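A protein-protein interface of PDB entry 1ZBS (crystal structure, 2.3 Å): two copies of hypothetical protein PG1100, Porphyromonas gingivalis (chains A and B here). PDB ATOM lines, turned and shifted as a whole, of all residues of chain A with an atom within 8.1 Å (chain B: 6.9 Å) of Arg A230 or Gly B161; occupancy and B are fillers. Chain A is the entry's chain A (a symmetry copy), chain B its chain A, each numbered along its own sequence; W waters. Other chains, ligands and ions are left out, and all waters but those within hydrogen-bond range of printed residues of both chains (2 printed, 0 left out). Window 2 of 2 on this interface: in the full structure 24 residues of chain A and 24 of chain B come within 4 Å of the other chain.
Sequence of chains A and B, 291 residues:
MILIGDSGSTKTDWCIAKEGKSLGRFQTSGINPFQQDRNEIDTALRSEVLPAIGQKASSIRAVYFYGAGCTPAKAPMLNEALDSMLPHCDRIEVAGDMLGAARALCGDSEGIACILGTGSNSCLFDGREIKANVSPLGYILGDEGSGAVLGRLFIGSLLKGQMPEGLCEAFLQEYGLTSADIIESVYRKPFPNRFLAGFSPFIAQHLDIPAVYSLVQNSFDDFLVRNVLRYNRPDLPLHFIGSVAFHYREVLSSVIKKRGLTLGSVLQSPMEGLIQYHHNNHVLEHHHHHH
Leu B159 touches Leu A137 (CB to CD2, 3.7 Å).
Leu A137 touches Lys B160.
NE2 of Gln B162 touches CG1 of Val A225 (3.6 Å).
C of Gly B156 touches NH2 of Arg A226, 3.3 Å away.
Arg A226 touches Lys B160 (O to CD, 3.5 Å).
Gln B162 touches Arg A226.
No position is printed for both chains.
Hydrophobic or aromatic side chains of chain B within 4 Å of the printed part of chain A: Leu B159.
Of the 17 printed residues of chain A, 5 touch a printed residue of chain B.
Printed residues of chain A that touch a printed residue of chain B: Leu A137, Val A225, Arg A226, Asn A227 and Arg A230.
Among the printed residues, no Asp or Glu carboxylate lies within 4 Å of a Lys or Arg side-chain nitrogen of the other chain.
The backbone carbonyl oxygen of Gly B161 lies within hydrogen-bond range of the guanidinium group of Arg A230, at 2.6 Å.
The side-chain amide oxygen of Asn A227 lies within hydrogen-bond range of the side-chain amino group of Lys B160 (3.0 Å).
The backbone NH (N) of Ser B157 lies close to the guanidinium group (NH2) of Arg A226, 3.0 Å away.
OG of Ser A122 is in hydrogen-bond range of O of Asn A227 (3.0 Å).
O of Lys B160 sits close to OE1 of Gln B162 (2.9 Å).
The backbone carbonyl oxygen (O) of Phe A223 is in hydrogen-bond range of the side-chain amide nitrogen (ND2) of Asn A227 (2.8 Å).
O of Arg A230 lies within hydrogen-bond range of ND2 of Asn A232, 3.4 Å away.
O of Ser B157 lies within hydrogen-bond range of N of Gln B162 (2.8 Å).
Of chain B, only Gly B161 (2.6 Å) comes within 4 Å of Arg A230.
Of the printed residues of chain A, Gly B161 touches Arg A230.
Of the printed residues of chain A, Lys B160 touches Leu A137 (3.4 Å), Arg A226 (3.5 Å) and Asn A227 (3.0 Å).
Of the printed residues of chain A, Gly B156 touches Arg A226.
Met B163 touches none of the printed residues of chain A.
Glu B165 touches none of the printed residues of chain A.
The nearest printed residue of chain A that does not touch Ser B157 is Leu A137 (6.1 Å).
Water W1 lies within hydrogen-bond range of NH2 of Arg A226 and O of Gly B156.
Water W2 bridges the side-chain amide oxygen (OD1) of Asn A227 (3.3 Å) and the side-chain amino group (NZ) of Lys B160 (3.4 Å).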
ATOM      1  N   ILE A 112       2.546  -4.540 -24.962  1.00  0.00           N
ATOM      2  CA  ILE A 112       2.772  -3.153 -24.586  1.00  0.00           C
ATOM      3  C   ILE A 112       4.217  -2.801 -24.868  1.00  0.00           C
ATOM      4  O   ILE A 112       5.129  -3.457 -24.363  1.00  0.00           O
ATOM      5  CB  ILE A 112       2.486  -2.921 -23.094  1.00  0.00           C
ATOM      6  CG1 ILE A 112       1.004  -3.159 -22.808  1.00  0.00           C
ATOM      7  CG2 ILE A 112       2.896  -1.501 -22.695  1.00  0.00           C
ATOM      8  CD1 ILE A 112       0.658  -3.210 -21.330  1.00  0.00           C
ATOM      9  N   SER A 122       4.695   5.224 -24.493  1.00  0.00           N
ATOM     10  CA  SER A 122       4.121   3.892 -24.351  1.00  0.00           C
ATOM     11  C   SER A 122       2.944   3.730 -25.299  1.00  0.00           C
ATOM     12  O   SER A 122       2.393   4.715 -25.787  1.00  0.00           O
ATOM     13  CB  SER A 122       3.663   3.612 -22.904  1.00  0.00           C
ATOM     14  OG  SER A 122       2.533   4.383 -22.538  1.00  0.00           O
ATOM     15  N   LEU A 124      -0.255   0.486 -26.542  1.00  0.00           N
ATOM     16  CA  LEU A 124      -0.787  -0.858 -26.464  1.00  0.00           C
ATOM     17  C   LEU A 124      -0.768  -1.287 -27.927  1.00  0.00           C
ATOM     18  O   LEU A 124      -1.328  -0.597 -28.781  1.00  0.00           O
ATOM     19  CB  LEU A 124      -2.222  -0.837 -25.933  1.00  0.00           C
ATOM     20  CG  LEU A 124      -2.745  -2.031 -25.120  1.00  0.00           C
ATOM     21  CD1 LEU A 124      -4.255  -2.133 -25.351  1.00  0.00           C
ATOM     22  CD2 LEU A 124      -2.065  -3.325 -25.526  1.00  0.00           C
ATOM     23  N   ALA A 132      -3.784   1.885 -28.480  1.00  0.00           N
ATOM     24  CA  ALA A 132      -3.900   2.944 -27.479  1.00  0.00           C
ATOM     25  C   ALA A 132      -2.530   3.549 -27.163  1.00  0.00           C
ATOM     26  O   ALA A 132      -1.528   2.839 -27.141  1.00  0.00           O
ATOM     27  CB  ALA A 132      -4.545   2.394 -26.210  1.00  0.00           C
ATOM     28  N   VAL A 134      -0.581   6.707 -24.572  1.00  0.00           N
ATOM     29  CA  VAL A 134      -0.679   7.748 -23.559  1.00  0.00           C
ATOM     30  C   VAL A 134       0.301   8.846 -23.963  1.00  0.00           C
ATOM     31  O   VAL A 134       1.509   8.608 -23.990  1.00  0.00           O
ATOM     32  CB  VAL A 134      -0.321   7.188 -22.160  1.00  0.00           C
ATOM     33  CG1 VAL A 134      -0.295   8.302 -21.122  1.00  0.00           C
ATOM     34  CG2 VAL A 134      -1.323   6.120 -21.767  1.00  0.00           C
ATOM     35  N   LEU A 137       3.609  13.894 -22.970  1.00  0.00           N
ATOM     36  CA  LEU A 137       3.519  15.224 -22.384  1.00  0.00           C
ATOM     37  C   LEU A 137       4.825  16.010 -22.260  1.00  0.00           C
ATOM     38  O   LEU A 137       4.805  17.152 -21.811  1.00  0.00           O
ATOM     39  CB  LEU A 137       2.824  15.127 -21.010  1.00  0.00           C
ATOM     40  CG  LEU A 137       1.313  15.379 -20.956  1.00  0.00           C
ATOM     41  CD1 LEU A 137       0.647  14.839 -22.202  1.00  0.00           C
ATOM     42  CD2 LEU A 137       0.732  14.782 -19.701  1.00  0.00           C
ATOM     43  N   PHE A 223       6.491   6.128 -14.149  1.00  0.00           N
ATOM     44  CA  PHE A 223       6.232   5.902 -15.560  1.00  0.00           C
ATOM     45  C   PHE A 223       5.219   4.775 -15.729  1.00  0.00           C
ATOM     46  O   PHE A 223       4.260   4.908 -16.495  1.00  0.00           O
ATOM     47  CB  PHE A 223       7.519   5.567 -16.318  1.00  0.00           C
ATOM     48  CG  PHE A 223       7.274   5.051 -17.711  1.00  0.00           C
ATOM     49  CD1 PHE A 223       7.215   3.682 -17.954  1.00  0.00           C
ATOM     50  CD2 PHE A 223       7.059   5.929 -18.770  1.00  0.00           C
ATOM     51  CE1 PHE A 223       6.931   3.196 -19.231  1.00  0.00           C
ATOM     52  CE2 PHE A 223       6.773   5.457 -20.053  1.00  0.00           C
ATOM     53  CZ  PHE A 223       6.711   4.084 -20.287  1.00  0.00           C
ATOM     54  N   LEU A 224       5.412   3.674 -15.011  1.00  0.00           N
ATOM     55  CA  LEU A 224       4.486   2.549 -15.125  1.00  0.00           C
ATOM     56  C   LEU A 224       3.082   2.956 -14.706  1.00  0.00           C
ATOM     57  O   LEU A 224       2.107   2.735 -15.433  1.00  0.00           O
ATOM     58  CB  LEU A 224       4.956   1.379 -14.258  1.00  0.00           C
ATOM     59  CG  LEU A 224       6.264   0.757 -14.737  1.00  0.00           C
ATOM     60  CD1 LEU A 224       6.744  -0.286 -13.737  1.00  0.00           C
ATOM     61  CD2 LEU A 224       6.045   0.138 -16.110  1.00  0.00           C
ATOM     62  N   VAL A 225       2.992   3.565 -13.530  1.00  0.00           N
ATOM     63  CA  VAL A 225       1.719   4.007 -12.995  1.00  0.00           C
ATOM     64  C   VAL A 225       0.906   4.866 -13.968  1.00  0.00           C
ATOM     65  O   VAL A 225      -0.219   4.518 -14.320  1.00  0.00           O
ATOM     66  CB  VAL A 225       1.924   4.808 -11.689  1.00  0.00           C
ATOM     67  CG1 VAL A 225       0.579   5.314 -11.171  1.00  0.00           C
ATOM     68  CG2 VAL A 225       2.593   3.923 -10.632  1.00  0.00           C
ATOM     69  N   ARG A 226       1.487   5.976 -14.412  1.00  0.00           N
ATOM     70  CA  ARG A 226       0.796   6.904 -15.306  1.00  0.00           C
ATOM     71  C   ARG A 226       0.874   6.598 -16.794  1.00  0.00           C
ATOM     72  O   ARG A 226       0.310   7.334 -17.607  1.00  0.00           O
ATOM     73  CB  ARG A 226       1.336   8.307 -15.076  1.00  0.00           C
ATOM     74  CG  ARG A 226       1.465   8.651 -13.611  1.00  0.00           C
ATOM     75  CD  ARG A 226       2.631   9.588 -13.396  1.00  0.00           C
ATOM     76  NE  ARG A 226       2.358  10.941 -13.856  1.00  0.00           N
ATOM     77  CZ  ARG A 226       1.958  11.928 -13.057  1.00  0.00           C
ATOM     78  NH1 ARG A 226       1.783  11.706 -11.761  1.00  0.00           N
ATOM     79  NH2 ARG A 226       1.763  13.146 -13.547  1.00  0.00           N
ATOM     80  N   ASN A 227       1.565   5.526 -17.168  1.00  0.00           N
ATOM     81  CA  ASN A 227       1.698   5.217 -18.589  1.00  0.00           C
ATOM     82  C   ASN A 227       1.363   3.783 -18.993  1.00  0.00           C
ATOM     83  O   ASN A 227       0.985   3.538 -20.139  1.00  0.00           O
ATOM     84  CB  ASN A 227       3.125   5.563 -19.062  1.00  0.00           C
ATOM     85  CG  ASN A 227       3.458   7.045 -18.903  1.00  0.00           C
ATOM     86  OD1 ASN A 227       3.036   7.874 -19.706  1.00  0.00           O
ATOM     87  ND2 ASN A 227       4.211   7.381 -17.859  1.00  0.00           N
ATOM     88  N   VAL A 228       1.494   2.840 -18.066  1.00  0.00           N
ATOM     89  CA  VAL A 228       1.224   1.432 -18.374  1.00  0.00           C
ATOM     90  C   VAL A 228      -0.014   0.853 -17.680  1.00  0.00           C
ATOM     91  O   VAL A 228      -0.844   0.210 -18.321  1.00  0.00           O
ATOM     92  CB  VAL A 228       2.446   0.545 -18.012  1.00  0.00           C
ATOM     93  CG1 VAL A 228       2.146  -0.922 -18.299  1.00  0.00           C
ATOM     94  CG2 VAL A 228       3.656   1.005 -18.798  1.00  0.00           C
ATOM     95  N   LEU A 229      -0.140   1.070 -16.375  1.00  0.00           N
ATOM     96  CA  LEU A 229      -1.276   0.527 -15.651  1.00  0.00           C
ATOM     97  C   LEU A 229      -2.612   0.771 -16.343  1.00  0.00           C
ATOM     98  O   LEU A 229      -3.421  -0.151 -16.509  1.00  0.00           O
ATOM     99  CB  LEU A 229      -1.331   1.096 -14.240  1.00  0.00           C
ATOM    100  CG  LEU A 229      -0.260   0.586 -13.278  1.00  0.00           C
ATOM    101  CD1 LEU A 229      -0.672   1.000 -11.877  1.00  0.00           C
ATOM    102  CD2 LEU A 229      -0.126  -0.937 -13.364  1.00  0.00           C
ATOM    103  N   ARG A 230      -2.825   2.016 -16.756  1.00  0.00           N
ATOM    104  CA  ARG A 230      -4.062   2.437 -17.416  1.00  0.00           C
ATOM    105  C   ARG A 230      -4.477   1.616 -18.632  1.00  0.00           C
ATOM    106  O   ARG A 230      -5.591   1.772 -19.133  1.00  0.00           O
ATOM    107  CB  ARG A 230      -3.964   3.917 -17.806  1.00  0.00           C
ATOM    108  CG  ARG A 230      -4.273   4.882 -16.652  1.00  0.00           C
ATOM    109  CD  ARG A 230      -5.737   4.753 -16.235  1.00  0.00           C
ATOM    110  NE  ARG A 230      -6.211   5.844 -15.372  1.00  0.00           N
ATOM    111  CZ  ARG A 230      -7.501   6.083 -15.132  1.00  0.00           C
ATOM    112  NH1 ARG A 230      -8.439   5.322 -15.693  1.00  0.00           N
ATOM    113  NH2 ARG A 230      -7.858   7.060 -14.314  1.00  0.00           N
ATOM    114  N   TYR A 231      -3.596   0.755 -19.126  1.00  0.00           N
ATOM    115  CA  TYR A 231      -3.979  -0.054 -20.274  1.00  0.00           C
ATOM    116  C   TYR A 231      -4.813  -1.235 -19.787  1.00  0.00           C
ATOM    117  O   TYR A 231      -5.532  -1.859 -20.564  1.00  0.00           O
ATOM    118  CB  TYR A 231      -2.748  -0.543 -21.042  1.00  0.00           C
ATOM    119  CG  TYR A 231      -1.984   0.548 -21.768  1.00  0.00           C
ATOM    120  CD1 TYR A 231      -2.654   1.529 -22.501  1.00  0.00           C
ATOM    121  CD2 TYR A 231      -0.590   0.594 -21.726  1.00  0.00           C
ATOM    122  CE1 TYR A 231      -1.956   2.532 -23.175  1.00  0.00           C
ATOM    123  CE2 TYR A 231       0.120   1.593 -22.394  1.00  0.00           C
ATOM    124  CZ  TYR A 231      -0.569   2.558 -23.114  1.00  0.00           C
ATOM    125  OH  TYR A 231       0.126   3.552 -23.762  1.00  0.00           O
ATOM    126  N   ASN A 232      -4.717  -1.528 -18.493  1.00  0.00           N
ATOM    127  CA  ASN A 232      -5.475  -2.623 -17.882  1.00  0.00           C
ATOM    128  C   ASN A 232      -5.211  -3.979 -18.532  1.00  0.00           C
ATOM    129  O   ASN A 232      -6.146  -4.730 -18.810  1.00  0.00           O
ATOM    130  CB  ASN A 232      -6.978  -2.329 -17.949  1.00  0.00           C
ATOM    131  CG  ASN A 232      -7.355  -1.040 -17.238  1.00  0.00           C
ATOM    132  OD1 ASN A 232      -6.992  -0.830 -16.085  1.00  0.00           O
ATOM    133  ND2 ASN A 232      -8.100  -0.180 -17.924  1.00  0.00           N
ATOM    134  N   ARG A 233      -3.937  -4.287 -18.770  1.00  0.00           N
ATOM    135  CA  ARG A 233      -3.552  -5.549 -19.386  1.00  0.00           C
ATOM    136  C   ARG A 233      -2.271  -6.127 -18.762  1.00  0.00           C
ATOM    137  O   ARG A 233      -1.283  -6.373 -19.463  1.00  0.00           O
ATOM    138  CB  ARG A 233      -3.351  -5.352 -20.898  1.00  0.00           C
ATOM    139  CG  ARG A 233      -4.628  -5.063 -21.689  1.00  0.00           C
ATOM    140  CD  ARG A 233      -5.591  -6.245 -21.645  1.00  0.00           C
ATOM    141  NE  ARG A 233      -5.007  -7.460 -22.219  1.00  0.00           N
ATOM    142  CZ  ARG A 233      -4.915  -7.703 -23.525  1.00  0.00           C
ATOM    143  NH1 ARG A 233      -5.370  -6.823 -24.401  1.00  0.00           N
ATOM    144  NH2 ARG A 233      -4.358  -8.823 -23.962  1.00  0.00           N
ATOM    145  N   GLY B 156      -0.294  17.504 -15.134  1.00  0.00           N
ATOM    146  CA  GLY B 156       0.392  16.282 -15.527  1.00  0.00           C
ATOM    147  C   GLY B 156      -0.406  15.067 -15.081  1.00  0.00           C
ATOM    148  O   GLY B 156      -0.800  14.229 -15.895  1.00  0.00           O
ATOM    149  N   SER B 157      -0.658  14.973 -13.781  1.00  0.00           N
ATOM    150  CA  SER B 157      -1.413  13.849 -13.248  1.00  0.00           C
ATOM    151  C   SER B 157      -2.840  13.841 -13.788  1.00  0.00           C
ATOM    152  O   SER B 157      -3.421  12.786 -14.039  1.00  0.00           O
ATOM    153  CB  SER B 157      -1.448  13.922 -11.727  1.00  0.00           C
ATOM    154  OG  SER B 157      -2.020  15.149 -11.335  1.00  0.00           O
ATOM    155  N   LEU B 158      -3.414  15.023 -13.955  1.00  0.00           N
ATOM    156  CA  LEU B 158      -4.774  15.124 -14.474  1.00  0.00           C
ATOM    157  C   LEU B 158      -4.847  14.496 -15.875  1.00  0.00           C
ATOM    158  O   LEU B 158      -5.709  13.668 -16.162  1.00  0.00           O
ATOM    159  CB  LEU B 158      -5.170  16.594 -14.538  1.00  0.00           C
ATOM    160  CG  LEU B 158      -6.560  16.966 -15.028  1.00  0.00           C
ATOM    161  CD1 LEU B 158      -7.562  16.830 -13.890  1.00  0.00           C
ATOM    162  CD2 LEU B 158      -6.527  18.394 -15.527  1.00  0.00           C
ATOM    163  N   LEU B 159      -3.924  14.899 -16.735  1.00  0.00           N
ATOM    164  CA  LEU B 159      -3.869  14.411 -18.102  1.00  0.00           C
ATOM    165  C   LEU B 159      -3.575  12.918 -18.184  1.00  0.00           C
ATOM    166  O   LEU B 159      -3.947  12.262 -19.156  1.00  0.00           O
ATOM    167  CB  LEU B 159      -2.815  15.200 -18.876  1.00  0.00           C
ATOM    168  CG  LEU B 159      -3.301  16.179 -19.949  1.00  0.00           C
ATOM    169  CD1 LEU B 159      -4.743  16.614 -19.707  1.00  0.00           C
ATOM    170  CD2 LEU B 159      -2.355  17.364 -19.974  1.00  0.00           C
ATOM    171  N   LYS B 160      -2.931  12.374 -17.159  1.00  0.00           N
ATOM    172  CA  LYS B 160      -2.606  10.959 -17.159  1.00  0.00           C
ATOM    173  C   LYS B 160      -3.516  10.103 -16.287  1.00  0.00           C
ATOM    174  O   LYS B 160      -3.117   9.051 -15.778  1.00  0.00           O
ATOM    175  CB  LYS B 160      -1.140  10.776 -16.785  1.00  0.00           C
ATOM    176  CG  LYS B 160      -0.243  11.525 -17.753  1.00  0.00           C
ATOM    177  CD  LYS B 160       0.998  10.759 -18.115  1.00  0.00           C
ATOM    178  CE  LYS B 160       1.824  11.580 -19.080  1.00  0.00           C
ATOM    179  NZ  LYS B 160       3.112  10.906 -19.451  1.00  0.00           N
ATOM    180  N   GLY B 161      -4.748  10.574 -16.124  1.00  0.00           N
ATOM    181  CA  GLY B 161      -5.745   9.850 -15.365  1.00  0.00           C
ATOM    182  C   GLY B 161      -5.450   9.540 -13.917  1.00  0.00           C
ATOM    183  O   GLY B 161      -5.860   8.493 -13.420  1.00  0.00           O
ATOM    184  N   GLN B 162      -4.758  10.427 -13.218  1.00  0.00           N
ATOM    185  CA  GLN B 162      -4.470  10.155 -11.817  1.00  0.00           C
ATOM    186  C   GLN B 162      -5.470  10.859 -10.904  1.00  0.00           C
ATOM    187  O   GLN B 162      -5.400  10.739  -9.680  1.00  0.00           O
ATOM    188  CB  GLN B 162      -3.039  10.574 -11.479  1.00  0.00           C
ATOM    189  CG  GLN B 162      -1.995   9.849 -12.314  1.00  0.00           C
ATOM    190  CD  GLN B 162      -2.150   8.333 -12.259  1.00  0.00           C
ATOM    191  OE1 GLN B 162      -2.346   7.680 -13.288  1.00  0.00           O
ATOM    192  NE2 GLN B 162      -2.068   7.771 -11.063  1.00  0.00           N
ATOM    193  N   MET B 163      -6.409  11.582 -11.506  1.00  0.00           N
ATOM    194  CA  MET B 163      -7.436  12.298 -10.755  1.00  0.00           C
ATOM    195  C   MET B 163      -8.801  11.607 -10.932  1.00  0.00           C
ATOM    196  O   MET B 163      -8.972  10.777 -11.822  1.00  0.00           O
ATOM    197  CB  MET B 163      -7.515  13.753 -11.241  1.00  0.00           C
ATOM    198  CG  MET B 163      -6.265  14.601 -10.978  1.00  0.00           C
ATOM    199  SD  MET B 163      -6.029  15.107  -9.108  1.00  0.00           S
ATOM    200  CE  MET B 163      -4.167  14.624  -8.859  1.00  0.00           C
ATOM    201  N   PRO B 164      -9.789  11.932 -10.077  1.00  0.00           N
ATOM    202  CA  PRO B 164     -11.106  11.296 -10.216  1.00  0.00           C
ATOM    203  C   PRO B 164     -11.665  11.465 -11.629  1.00  0.00           C
ATOM    204  O   PRO B 164     -11.298  12.405 -12.336  1.00  0.00           O
ATOM    205  CB  PRO B 164     -11.941  12.018  -9.164  1.00  0.00           C
ATOM    206  CG  PRO B 164     -10.938  12.274  -8.084  1.00  0.00           C
ATOM    207  CD  PRO B 164      -9.756  12.795  -8.884  1.00  0.00           C
ATOM    208  N   GLU B 165     -12.543  10.552 -12.037  1.00  0.00           N
ATOM    209  CA  GLU B 165     -13.149  10.589 -13.368  1.00  0.00           C
ATOM    210  C   GLU B 165     -13.937  11.875 -13.546  1.00  0.00           C
ATOM    211  O   GLU B 165     -14.703  12.275 -12.667  1.00  0.00           O
ATOM    212  CB  GLU B 165     -14.084   9.382 -13.561  1.00  0.00           C
ATOM    213  CG  GLU B 165     -14.509   9.068 -15.018  1.00  0.00           C
ATOM    214  CD  GLU B 165     -15.513  10.065 -15.616  1.00  0.00           C
ATOM    215  OE1 GLU B 165     -16.561  10.332 -14.986  1.00  0.00           O
ATOM    216  OE2 GLU B 165     -15.255  10.563 -16.734  1.00  0.00           O
ATOM    217  N   CYS B 168     -10.657  15.856 -15.265  1.00  0.00           N
ATOM    218  CA  CYS B 168      -9.884  16.293 -16.414  1.00  0.00           C
ATOM    219  C   CYS B 168     -10.791  17.048 -17.365  1.00  0.00           C
ATOM    220  O   CYS B 168     -10.501  18.182 -17.739  1.00  0.00           O
ATOM    221  CB  CYS B 168      -9.260  15.091 -17.128  1.00  0.00           C
ATOM    222  SG  CYS B 168      -8.121  15.546 -18.448  1.00  0.00           S
HETATM  223  O   HOH W   1       2.329  13.110 -16.220  1.00  0.00           O
HETATM  224  O   HOH W   2       5.736   9.332 -20.845  1.00  0.00           O
